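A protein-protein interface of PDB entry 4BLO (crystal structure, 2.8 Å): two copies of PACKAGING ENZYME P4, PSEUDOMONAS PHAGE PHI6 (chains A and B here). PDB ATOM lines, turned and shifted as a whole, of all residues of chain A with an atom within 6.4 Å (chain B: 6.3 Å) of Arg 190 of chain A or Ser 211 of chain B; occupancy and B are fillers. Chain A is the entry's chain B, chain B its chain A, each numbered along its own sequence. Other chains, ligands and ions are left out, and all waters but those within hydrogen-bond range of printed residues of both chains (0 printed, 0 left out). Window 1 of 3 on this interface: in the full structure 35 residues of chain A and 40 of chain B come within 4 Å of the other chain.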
ATOM      1  N   THR A 128     -28.628 -21.722 -13.932  1.00  0.00           N
ATOM      2  CA  THR A 128     -27.780 -20.946 -13.021  1.00  0.00           C
ATOM      3  C   THR A 128     -28.434 -20.873 -11.656  1.00  0.00           C
ATOM      4  O   THR A 128     -29.633 -20.598 -11.550  1.00  0.00           O
ATOM      5  CB  THR A 128     -27.445 -19.555 -13.548  1.00  0.00           C
ATOM      6  OG1 THR A 128     -28.597 -18.964 -14.148  1.00  0.00           O
ATOM      7  CG2 THR A 128     -26.275 -19.572 -14.505  1.00  0.00           C
ATOM      8  N   TRP A 148     -11.994 -22.905 -12.638  1.00  0.00           N
ATOM      9  CA  TRP A 148     -11.758 -22.200 -13.878  1.00  0.00           C
ATOM     10  C   TRP A 148     -13.010 -21.437 -14.317  1.00  0.00           C
ATOM     11  O   TRP A 148     -14.098 -22.016 -14.384  1.00  0.00           O
ATOM     12  CB  TRP A 148     -11.354 -23.239 -14.930  1.00  0.00           C
ATOM     13  CG  TRP A 148     -10.863 -22.717 -16.254  1.00  0.00           C
ATOM     14  CD1 TRP A 148     -10.064 -21.628 -16.476  1.00  0.00           C
ATOM     15  CD2 TRP A 148     -11.020 -23.361 -17.520  1.00  0.00           C
ATOM     16  NE1 TRP A 148      -9.787 -21.513 -17.818  1.00  0.00           N
ATOM     17  CE2 TRP A 148     -10.337 -22.580 -18.478  1.00  0.00           C
ATOM     18  CE3 TRP A 148     -11.680 -24.527 -17.943  1.00  0.00           C
ATOM     19  CZ2 TRP A 148     -10.308 -22.923 -19.834  1.00  0.00           C
ATOM     20  CZ3 TRP A 148     -11.629 -24.879 -19.282  1.00  0.00           C
ATOM     21  CH2 TRP A 148     -10.956 -24.077 -20.210  1.00  0.00           C
ATOM     22  N   GLY A 149     -12.832 -20.149 -14.622  1.00  0.00           N
ATOM     23  CA  GLY A 149     -13.887 -19.257 -15.105  1.00  0.00           C
ATOM     24  C   GLY A 149     -15.077 -19.073 -14.185  1.00  0.00           C
ATOM     25  O   GLY A 149     -16.213 -18.897 -14.639  1.00  0.00           O
ATOM     26  N   GLU A 150     -14.809 -19.089 -12.878  1.00  0.00           N
ATOM     27  CA  GLU A 150     -15.810 -18.937 -11.835  1.00  0.00           C
ATOM     28  C   GLU A 150     -15.422 -17.797 -10.935  1.00  0.00           C
ATOM     29  O   GLU A 150     -14.240 -17.616 -10.626  1.00  0.00           O
ATOM     30  CB  GLU A 150     -15.963 -20.250 -11.051  1.00  0.00           C
ATOM     31  CG  GLU A 150     -16.696 -21.334 -11.831  1.00  0.00           C
ATOM     32  CD  GLU A 150     -18.127 -20.995 -12.213  1.00  0.00           C
ATOM     33  OE1 GLU A 150     -18.896 -20.588 -11.310  1.00  0.00           O
ATOM     34  OE2 GLU A 150     -18.475 -21.130 -13.412  1.00  0.00           O
ATOM     35  N   VAL A 151     -16.411 -17.018 -10.508  1.00  0.00           N
ATOM     36  CA  VAL A 151     -16.165 -15.858  -9.660  1.00  0.00           C
ATOM     37  C   VAL A 151     -15.734 -16.315  -8.233  1.00  0.00           C
ATOM     38  O   VAL A 151     -15.831 -17.507  -7.916  1.00  0.00           O
ATOM     39  CB  VAL A 151     -17.402 -14.925  -9.690  1.00  0.00           C
ATOM     40  CG1 VAL A 151     -18.432 -15.281  -8.618  1.00  0.00           C
ATOM     41  CG2 VAL A 151     -16.991 -13.471  -9.603  1.00  0.00           C
ATOM     42  N   SER A 188     -15.426 -24.335 -13.450  1.00  0.00           N
ATOM     43  CA  SER A 188     -16.211 -25.030 -14.491  1.00  0.00           C
ATOM     44  C   SER A 188     -15.486 -25.007 -15.849  1.00  0.00           C
ATOM     45  O   SER A 188     -14.284 -24.714 -15.920  1.00  0.00           O
ATOM     46  CB  SER A 188     -17.626 -24.446 -14.619  1.00  0.00           C
ATOM     47  OG  SER A 188     -17.679 -23.037 -14.763  1.00  0.00           O
ATOM     48  N   VAL A 189     -16.244 -25.352 -16.915  1.00  0.00           N
ATOM     49  CA  VAL A 189     -15.815 -25.452 -18.311  1.00  0.00           C
ATOM     50  C   VAL A 189     -16.504 -24.314 -19.136  1.00  0.00           C
ATOM     51  O   VAL A 189     -16.401 -24.271 -20.373  1.00  0.00           O
ATOM     52  CB  VAL A 189     -16.071 -26.898 -18.861  1.00  0.00           C
ATOM     53  CG1 VAL A 189     -17.556 -27.227 -18.977  1.00  0.00           C
ATOM     54  CG2 VAL A 189     -15.371 -27.126 -20.181  1.00  0.00           C
ATOM     55  N   ARG A 190     -17.152 -23.364 -18.430  1.00  0.00           N
ATOM     56  CA  ARG A 190     -17.761 -22.174 -19.024  1.00  0.00           C
ATOM     57  C   ARG A 190     -16.786 -21.421 -19.946  1.00  0.00           C
ATOM     58  O   ARG A 190     -17.262 -20.929 -20.960  1.00  0.00           O
ATOM     59  CB  ARG A 190     -18.243 -21.206 -17.937  1.00  0.00           C
ATOM     60  CG  ARG A 190     -19.535 -21.594 -17.237  1.00  0.00           C
ATOM     61  CD  ARG A 190     -20.247 -20.356 -16.689  1.00  0.00           C
ATOM     62  NE  ARG A 190     -19.414 -19.533 -15.801  1.00  0.00           N
ATOM     63  CZ  ARG A 190     -19.686 -18.270 -15.485  1.00  0.00           C
ATOM     64  NH1 ARG A 190     -20.760 -17.671 -15.984  1.00  0.00           N
ATOM     65  NH2 ARG A 190     -18.888 -17.597 -14.664  1.00  0.00           N
ATOM     66  N   PRO A 191     -15.452 -21.309 -19.660  1.00  0.00           N
ATOM     67  CA  PRO A 191     -14.568 -20.540 -20.551  1.00  0.00           C
ATOM     68  C   PRO A 191     -14.425 -21.114 -21.960  1.00  0.00           C
ATOM     69  O   PRO A 191     -14.161 -20.367 -22.905  1.00  0.00           O
ATOM     70  CB  PRO A 191     -13.238 -20.580 -19.811  1.00  0.00           C
ATOM     71  CG  PRO A 191     -13.616 -20.732 -18.390  1.00  0.00           C
ATOM     72  CD  PRO A 191     -14.695 -21.737 -18.467  1.00  0.00           C
ATOM     73  N   LEU A 192     -14.635 -22.415 -22.110  1.00  0.00           N
ATOM     74  CA  LEU A 192     -14.579 -23.087 -23.401  1.00  0.00           C
ATOM     75  C   LEU A 192     -15.963 -22.963 -24.044  1.00  0.00           C
ATOM     76  O   LEU A 192     -16.079 -22.438 -25.153  1.00  0.00           O
ATOM     77  CB  LEU A 192     -14.128 -24.552 -23.209  1.00  0.00           C
ATOM     78  CG  LEU A 192     -14.500 -25.619 -24.255  1.00  0.00           C
ATOM     79  CD1 LEU A 192     -13.699 -25.430 -25.539  1.00  0.00           C
ATOM     80  CD2 LEU A 192     -14.306 -27.045 -23.659  1.00  0.00           C
ATOM     81  N   LEU A 193     -17.017 -23.337 -23.291  1.00  0.00           N
ATOM     82  CA  LEU A 193     -18.395 -23.316 -23.796  1.00  0.00           C
ATOM     83  C   LEU A 193     -18.820 -21.957 -24.277  1.00  0.00           C
ATOM     84  O   LEU A 193     -19.359 -21.856 -25.379  1.00  0.00           O
ATOM     85  CB  LEU A 193     -19.419 -23.834 -22.776  1.00  0.00           C
ATOM     86  CG  LEU A 193     -19.121 -25.191 -22.116  1.00  0.00           C
ATOM     87  CD1 LEU A 193     -20.222 -25.575 -21.125  1.00  0.00           C
ATOM     88  CD2 LEU A 193     -18.774 -26.299 -23.157  1.00  0.00           C
ATOM     89  N   PHE A 194     -18.574 -20.909 -23.492  1.00  0.00           N
ATOM     90  CA  PHE A 194     -18.999 -19.546 -23.861  1.00  0.00           C
ATOM     91  C   PHE A 194     -18.175 -18.969 -25.017  1.00  0.00           C
ATOM     92  O   PHE A 194     -18.580 -17.966 -25.583  1.00  0.00           O
ATOM     93  CB  PHE A 194     -18.968 -18.611 -22.635  1.00  0.00           C
ATOM     94  CG  PHE A 194     -20.053 -18.869 -21.605  1.00  0.00           C
ATOM     95  CD1 PHE A 194     -20.904 -19.970 -21.717  1.00  0.00           C
ATOM     96  CD2 PHE A 194     -20.227 -18.016 -20.528  1.00  0.00           C
ATOM     97  CE1 PHE A 194     -21.896 -20.209 -20.766  1.00  0.00           C
ATOM     98  CE2 PHE A 194     -21.231 -18.251 -19.589  1.00  0.00           C
ATOM     99  CZ  PHE A 194     -22.054 -19.346 -19.714  1.00  0.00           C
ATOM    100  N   ARG A 195     -17.062 -19.619 -25.392  1.00  0.00           N
ATOM    101  CA  ARG A 195     -16.222 -19.165 -26.485  1.00  0.00           C
ATOM    102  C   ARG A 195     -16.348 -20.092 -27.703  1.00  0.00           C
ATOM    103  O   ARG A 195     -15.673 -19.853 -28.703  1.00  0.00           O
ATOM    104  CB  ARG A 195     -14.765 -18.995 -26.032  1.00  0.00           C
ATOM    105  CG  ARG A 195     -14.542 -17.670 -25.337  1.00  0.00           C
ATOM    106  CD  ARG A 195     -13.193 -17.565 -24.682  1.00  0.00           C
ATOM    107  NE  ARG A 195     -13.077 -16.333 -23.904  1.00  0.00           N
ATOM    108  CZ  ARG A 195     -12.885 -16.294 -22.595  1.00  0.00           C
ATOM    109  NH1 ARG A 195     -12.787 -17.420 -21.898  1.00  0.00           N
ATOM    110  NH2 ARG A 195     -12.789 -15.129 -21.968  1.00  0.00           N
ATOM    111  N   VAL A 230     -18.657 -29.585 -14.431  1.00  0.00           N
ATOM    112  CA  VAL A 230     -19.945 -28.907 -14.346  1.00  0.00           C
ATOM    113  C   VAL A 230     -20.107 -28.212 -15.711  1.00  0.00           C
ATOM    114  O   VAL A 230     -19.236 -27.430 -16.113  1.00  0.00           O
ATOM    115  CB  VAL A 230     -20.227 -27.992 -13.085  1.00  0.00           C
ATOM    116  CG1 VAL A 230     -19.179 -28.135 -11.998  1.00  0.00           C
ATOM    117  CG2 VAL A 230     -20.475 -26.524 -13.438  1.00  0.00           C
ATOM    118  N   VAL A 231     -21.140 -28.608 -16.473  1.00  0.00           N
ATOM    119  CA  VAL A 231     -21.373 -28.052 -17.811  1.00  0.00           C
ATOM    120  C   VAL A 231     -22.639 -27.169 -17.759  1.00  0.00           C
ATOM    121  O   VAL A 231     -23.742 -27.651 -17.480  1.00  0.00           O
ATOM    122  CB  VAL A 231     -21.375 -29.129 -18.969  1.00  0.00           C
ATOM    123  CG1 VAL A 231     -20.132 -30.030 -18.908  1.00  0.00           C
ATOM    124  CG2 VAL A 231     -22.631 -29.983 -18.980  1.00  0.00           C
ATOM    125  N   ASN A 232     -22.442 -25.855 -17.919  1.00  0.00           N
ATOM    126  CA  ASN A 232     -23.534 -24.880 -17.863  1.00  0.00           C
ATOM    127  C   ASN A 232     -23.549 -24.000 -19.153  1.00  0.00           C
ATOM    128  O   ASN A 232     -23.084 -22.857 -19.140  1.00  0.00           O
ATOM    129  CB  ASN A 232     -23.427 -24.023 -16.580  1.00  0.00           C
ATOM    130  CG  ASN A 232     -24.631 -23.153 -16.260  1.00  0.00           C
ATOM    131  OD1 ASN A 232     -24.492 -22.107 -15.615  1.00  0.00           O
ATOM    132  ND2 ASN A 232     -25.842 -23.562 -16.655  1.00  0.00           N
ATOM    133  N   PRO A 233     -24.067 -24.504 -20.286  1.00  0.00           N
ATOM    134  CA  PRO A 233     -24.099 -23.662 -21.502  1.00  0.00           C
ATOM    135  C   PRO A 233     -25.323 -22.748 -21.553  1.00  0.00           C
ATOM    136  O   PRO A 233     -26.345 -23.070 -20.945  1.00  0.00           O
ATOM    137  CB  PRO A 233     -24.131 -24.683 -22.641  1.00  0.00           C
ATOM    138  CG  PRO A 233     -24.640 -25.956 -22.029  1.00  0.00           C
ATOM    139  CD  PRO A 233     -24.659 -25.835 -20.534  1.00  0.00           C
ATOM    140  N   MET A 234     -25.218 -21.609 -22.271  1.00  0.00           N
ATOM    141  CA  MET A 234     -26.313 -20.640 -22.409  1.00  0.00           C
ATOM    142  C   MET A 234     -27.460 -21.256 -23.204  1.00  0.00           C
ATOM    143  O   MET A 234     -27.415 -21.335 -24.438  1.00  0.00           O
ATOM    144  CB  MET A 234     -25.835 -19.320 -23.041  1.00  0.00           C
ATOM    145  CG  MET A 234     -25.202 -18.356 -22.058  1.00  0.00           C
ATOM    146  SD  MET A 234     -26.306 -17.853 -20.700  1.00  0.00           S
ATOM    147  CE  MET A 234     -25.565 -18.749 -19.395  1.00  0.00           C
ATOM    148  N   GLN B  28      -9.027 -12.465 -22.598  1.00  0.00           N
ATOM    149  CA  GLN B  28      -9.445 -13.026 -23.865  1.00  0.00           C
ATOM    150  C   GLN B  28     -10.931 -12.779 -24.063  1.00  0.00           C
ATOM    151  O   GLN B  28     -11.703 -12.832 -23.092  1.00  0.00           O
ATOM    152  CB  GLN B  28      -9.128 -14.518 -23.931  1.00  0.00           C
ATOM    153  CG  GLN B  28      -9.165 -15.098 -25.347  1.00  0.00           C
ATOM    154  CD  GLN B  28      -9.370 -16.592 -25.372  1.00  0.00           C
ATOM    155  OE1 GLN B  28      -9.744 -17.221 -24.383  1.00  0.00           O
ATOM    156  NE2 GLN B  28      -9.131 -17.192 -26.507  1.00  0.00           N
ATOM    157  N   SER B  99      -8.852 -17.768 -18.932  1.00  0.00           N
ATOM    158  CA  SER B  99      -9.705 -17.152 -17.922  1.00  0.00           C
ATOM    159  C   SER B  99      -8.809 -16.664 -16.835  1.00  0.00           C
ATOM    160  O   SER B  99      -7.823 -17.336 -16.530  1.00  0.00           O
ATOM    161  CB  SER B  99     -10.747 -18.128 -17.400  1.00  0.00           C
ATOM    162  OG  SER B  99     -11.781 -18.201 -18.360  1.00  0.00           O
ATOM    163  N   ALA B 207     -22.543 -15.184 -25.467  1.00  0.00           N
ATOM    164  CA  ALA B 207     -22.161 -15.920 -24.265  1.00  0.00           C
ATOM    165  C   ALA B 207     -20.875 -15.398 -23.623  1.00  0.00           C
ATOM    166  O   ALA B 207     -20.820 -15.355 -22.399  1.00  0.00           O
ATOM    167  CB  ALA B 207     -22.020 -17.389 -24.583  1.00  0.00           C
ATOM    168  N   VAL B 208     -19.877 -14.955 -24.428  1.00  0.00           N
ATOM    169  CA  VAL B 208     -18.568 -14.465 -23.967  1.00  0.00           C
ATOM    170  C   VAL B 208     -18.729 -13.222 -23.061  1.00  0.00           C
ATOM    171  O   VAL B 208     -17.795 -12.855 -22.340  1.00  0.00           O
ATOM    172  CB  VAL B 208     -17.586 -14.223 -25.156  1.00  0.00           C
ATOM    173  CG1 VAL B 208     -17.895 -12.921 -25.895  1.00  0.00           C
ATOM    174  CG2 VAL B 208     -16.126 -14.264 -24.699  1.00  0.00           C
ATOM    175  N   PHE B 209     -19.924 -12.606 -23.071  1.00  0.00           N
ATOM    176  CA  PHE B 209     -20.250 -11.460 -22.222  1.00  0.00           C
ATOM    177  C   PHE B 209     -20.164 -11.863 -20.744  1.00  0.00           C
ATOM    178  O   PHE B 209     -19.588 -11.127 -19.947  1.00  0.00           O
ATOM    179  CB  PHE B 209     -21.645 -10.905 -22.582  1.00  0.00           C
ATOM    180  CG  PHE B 209     -22.327 -10.068 -21.524  1.00  0.00           C
ATOM    181  CD1 PHE B 209     -21.931  -8.755 -21.289  1.00  0.00           C
ATOM    182  CD2 PHE B 209     -23.379 -10.585 -20.778  1.00  0.00           C
ATOM    183  CE1 PHE B 209     -22.560  -7.983 -20.306  1.00  0.00           C
ATOM    184  CE2 PHE B 209     -24.016  -9.809 -19.803  1.00  0.00           C
ATOM    185  CZ  PHE B 209     -23.601  -8.515 -19.573  1.00  0.00           C
ATOM    186  N   TYR B 210     -20.703 -13.041 -20.400  1.00  0.00           N
ATOM    187  CA  TYR B 210     -20.713 -13.576 -19.038  1.00  0.00           C
ATOM    188  C   TYR B 210     -19.315 -14.003 -18.593  1.00  0.00           C
ATOM    189  O   TYR B 210     -18.954 -13.807 -17.423  1.00  0.00           O
ATOM    190  CB  TYR B 210     -21.699 -14.733 -18.917  1.00  0.00           C
ATOM    191  CG  TYR B 210     -23.102 -14.349 -19.322  1.00  0.00           C
ATOM    192  CD1 TYR B 210     -23.909 -13.590 -18.480  1.00  0.00           C
ATOM    193  CD2 TYR B 210     -23.625 -14.744 -20.550  1.00  0.00           C
ATOM    194  CE1 TYR B 210     -25.193 -13.204 -18.862  1.00  0.00           C
ATOM    195  CE2 TYR B 210     -24.918 -14.387 -20.931  1.00  0.00           C
ATOM    196  CZ  TYR B 210     -25.702 -13.623 -20.078  1.00  0.00           C
ATOM    197  OH  TYR B 210     -26.985 -13.290 -20.428  1.00  0.00           O
ATOM    198  N   SER B 211     -18.518 -14.545 -19.534  1.00  0.00           N
ATOM    199  CA  SER B 211     -17.133 -14.925 -19.278  1.00  0.00           C
ATOM    200  C   SER B 211     -16.292 -13.680 -18.999  1.00  0.00           C
ATOM    201  O   SER B 211     -15.512 -13.685 -18.045  1.00  0.00           O
ATOM    202  CB  SER B 211     -16.563 -15.722 -20.445  1.00  0.00           C
ATOM    203  OG  SER B 211     -16.873 -17.091 -20.277  1.00  0.00           O
ATOM    204  N   LEU B 212     -16.510 -12.593 -19.778  1.00  0.00           N
ATOM    205  CA  LEU B 212     -15.811 -11.321 -19.606  1.00  0.00           C
ATOM    206  C   LEU B 212     -16.081 -10.705 -18.234  1.00  0.00           C
ATOM    207  O   LEU B 212     -15.128 -10.240 -17.613  1.00  0.00           O
ATOM    208  CB  LEU B 212     -16.165 -10.319 -20.705  1.00  0.00           C
ATOM    209  CG  LEU B 212     -15.020  -9.889 -21.633  1.00  0.00           C
ATOM    210  CD1 LEU B 212     -15.552  -9.007 -22.759  1.00  0.00           C
ATOM    211  CD2 LEU B 212     -13.919  -9.127 -20.873  1.00  0.00           C
ATOM    212  N   LEU B 213     -17.349 -10.736 -17.747  1.00  0.00           N
ATOM    213  CA  LEU B 213     -17.713 -10.220 -16.424  1.00  0.00           C
ATOM    214  C   LEU B 213     -16.960 -10.965 -15.307  1.00  0.00           C
ATOM    215  O   LEU B 213     -16.468 -10.329 -14.379  1.00  0.00           O
ATOM    216  CB  LEU B 213     -19.221 -10.323 -16.182  1.00  0.00           C
ATOM    217  CG  LEU B 213     -20.124  -9.269 -16.820  1.00  0.00           C
ATOM    218  CD1 LEU B 213     -21.580  -9.658 -16.679  1.00  0.00           C
ATOM    219  CD2 LEU B 213     -19.937  -7.918 -16.180  1.00  0.00           C
ATOM    220  N   THR B 214     -16.853 -12.305 -15.416  1.00  0.00           N
ATOM    221  CA  THR B 214     -16.146 -13.166 -14.462  1.00  0.00           C
ATOM    222  C   THR B 214     -14.650 -12.844 -14.485  1.00  0.00           C
ATOM    223  O   THR B 214     -14.045 -12.718 -13.422  1.00  0.00           O
ATOM    224  CB  THR B 214     -16.410 -14.659 -14.770  1.00  0.00           C
ATOM    225  OG1 THR B 214     -17.804 -14.914 -14.706  1.00  0.00           O
ATOM    226  CG2 THR B 214     -15.727 -15.587 -13.794  1.00  0.00           C
ATOM    227  N   ASP B 215     -14.064 -12.714 -15.699  1.00  0.00           N
ATOM    228  CA  ASP B 215     -12.644 -12.401 -15.909  1.00  0.00           C
ATOM    229  C   ASP B 215     -12.326 -11.014 -15.348  1.00  0.00           C
ATOM    230  O   ASP B 215     -11.288 -10.840 -14.718  1.00  0.00           O
ATOM    231  CB  ASP B 215     -12.278 -12.502 -17.405  1.00  0.00           C
ATOM    232  CG  ASP B 215     -12.107 -13.920 -17.947  1.00  0.00           C
ATOM    233  OD1 ASP B 215     -12.219 -14.887 -17.152  1.00  0.00           O
ATOM    234  OD2 ASP B 215     -11.829 -14.063 -19.167  1.00  0.00           O
ATOM    235  N   ILE B 216     -13.238 -10.044 -15.537  1.00  0.00           N
ATOM    236  CA  ILE B 216     -13.082  -8.690 -15.016  1.00  0.00           C
ATOM    237  C   ILE B 216     -13.205  -8.750 -13.476  1.00  0.00           C
ATOM    238  O   ILE B 216     -12.362  -8.189 -12.779  1.00  0.00           O
ATOM    239  CB  ILE B 216     -14.098  -7.708 -15.669  1.00  0.00           C
ATOM    240  CG1 ILE B 216     -13.687  -7.342 -17.097  1.00  0.00           C
ATOM    241  CG2 ILE B 216     -14.248  -6.434 -14.842  1.00  0.00           C
ATOM    242  CD1 ILE B 216     -14.872  -6.788 -17.958  1.00  0.00           C
ATOM    243  N   GLN B 246     -28.267 -14.622 -14.766  1.00  0.00           N
ATOM    244  CA  GLN B 246     -27.054 -15.186 -15.346  1.00  0.00           C
ATOM    245  C   GLN B 246     -25.829 -14.370 -14.938  1.00  0.00           C
ATOM    246  O   GLN B 246     -24.756 -14.936 -14.735  1.00  0.00           O
ATOM    247  CB  GLN B 246     -27.169 -15.247 -16.877  1.00  0.00           C
ATOM    248  CG  GLN B 246     -28.331 -16.106 -17.403  1.00  0.00           C
ATOM    249  CD  GLN B 246     -28.218 -17.579 -17.091  1.00  0.00           C
ATOM    250  OE1 GLN B 246     -27.136 -18.164 -17.119  1.00  0.00           O
ATOM    251  NE2 GLN B 246     -29.334 -18.212 -16.803  1.00  0.00           N
ATOM    252  N   ALA B 249     -24.389 -15.055 -11.360  1.00  0.00           N
ATOM    253  CA  ALA B 249     -23.515 -16.222 -11.351  1.00  0.00           C
ATOM    254  C   ALA B 249     -22.117 -15.891 -11.925  1.00  0.00           C
ATOM    255  O   ALA B 249     -21.225 -16.749 -11.900  1.00  0.00           O
ATOM    256  CB  ALA B 249     -24.163 -17.337 -12.161  1.00  0.00           C
ATOM    257  N   SER B 250     -21.926 -14.654 -12.418  1.00  0.00           N
ATOM    258  CA  SER B 250     -20.692 -14.203 -13.060  1.00  0.00           C
ATOM    259  C   SER B 250     -20.024 -13.010 -12.343  1.00  0.00           C
ATOM    260  O   SER B 250     -18.938 -12.591 -12.754  1.00  0.00           O
ATOM    261  CB  SER B 250     -20.985 -13.814 -14.508  1.00  0.00           C
ATOM    262  OG  SER B 250     -21.555 -14.895 -15.234  1.00  0.00           O
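NH2 of Arg 195 of chain A sits at hydrogen-bond distance from O of Gln 28 of chain B (2.8 Å).
O of Phe 194 of chain A lies within hydrogen-bond range of N of Val 208 of chain B.
The side-chain hydroxyl (OG1) of Thr 214 of chain B sits at hydrogen-bond distance from the guanidinium group (NH2) of Arg 190 of chain A.
OD2 of Asp 215 of chain B is in salt-bridge range of NH2 of Arg 195 of chain A (3.1 Å).
The side-chain amide nitrogen (NE2) of Gln 246 of chain B sits at hydrogen-bond distance from the side-chain hydroxyl (OG1) of Thr 128 of chain A (2.9 Å).
The side-chain sulfur (SD) of Met 234 of chain A sits close to the side-chain amide oxygen (OE1) of Gln 246 of chain B, 3.7 Å away.
OG of Ser 250 of chain B is in hydrogen-bond range of NH1 of Arg 190 of chain A, 3.0 Å away.
The backbone carbonyl oxygen of Tyr 210 of chain B is in hydrogen-bond range of the side-chain hydroxyl of Thr 214 of chain B (3.2 Å).
O of Ser 250 of chain B lies within hydrogen-bond range of OG1 of Thr 214 of chain B, at 3.2 Å.
The backbone carbonyl oxygen (O) of Trp 148 of chain A lies within hydrogen-bond range of the backbone NH (N) of Ser 188 of chain A, 2.8 Å away.
The side-chain carboxylate (OE2) of Glu 150 of chain A sits at hydrogen-bond distance from the side-chain hydroxyl (OG) of Ser 188 of chain A, at 2.5 Å.
NE of Arg 190 of chain A is in salt-bridge range of OE2 of Glu 150 of chain A, 3.0 Å away.
The backbone carbonyl oxygen (O) of Pro 191 of chain A is in hydrogen-bond range of the guanidinium group (NH1) of Arg 195 of chain A (3.4 Å).
O of Gly 149 of chain A touches CG2 of Thr 214 of chain B, 3.5 Å away.
C of Glu 150 of chain A touches CG2 of Thr 214 of chain B, 3.6 Å away.
Thr 214 of chain B touches Val 151 of chain A.
Ser 250 of chain B touches Val 151 of chain A (O to CG2, 3.8 Å).
Arg 190 of chain A touches Ala 249 of chain B (NH2 to O, 3.7 Å).
Pro 191 of chain A touches Ser 99 of chain B.
CD2 of Phe 194 of chain A touches O of Ala 207 of chain B (3.3 Å).
CE2 of Phe 194 of chain A touches CB of Tyr 210 of chain B, 3.6 Å away.
NH1 of Arg 195 of chain A touches OG of Ser 99 of chain B, 3.8 Å away.
NE of Arg 195 of chain A touches CG2 of Val 208 of chain B, 3.8 Å away.
Arg 190 of chain A touches just these residues of chain B: Ser 211 (3.9 Å), Thr 214 (2.9 Å), Ala 249 (3.7 Å) and Ser 250 (3.0 Å).
Printed residues of chain B within 4 Å of Arg 195 of chain A: Gln 28 (2.8 Å), Ser 99 (3.8 Å), Val 208 (3.8 Å) and Asp 215 (3.1 Å).
Printed residues of chain B within 4 Å of Met 234 of chain A: Tyr 210 (3.7 Å) and Gln 246 (2.8 Å).
Of the printed residues of chain A, Ser 211 of chain B touches Arg 190 (3.9 Å) and Phe 194 (3.5 Å).
The nearest residue of chain B that does not touch Arg 190 of chain A is Tyr 210 of chain B (4.3 Å).
Printed residues of chain A that touch a printed residue of chain B: Thr 128, Trp 148, Gly 149, Glu 150, Val 151, Arg 190, Pro 191, Phe 194, Arg 195 and Met 234.
Hydrophobic or aromatic side chains of chain A that line the printed part of chain B: Trp 148, Val 151, Pro 191, Phe 194 and Met 234.
Of the 15 printed residues of chain B, 11 touch a printed residue of chain A.
Along chain B the printed residues that touch a printed residue of chain A span positions 28 to 250.
Among the printed residues, 22 pairs touch across the chains.
Among the printed residues, Asp or Glu carboxylates within 4 Å of a Lys or Arg side-chain nitrogen of the other chain: Arg 195 of chain A with Asp 215 of chain B (3.1 Å).
No position is printed for both chains.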
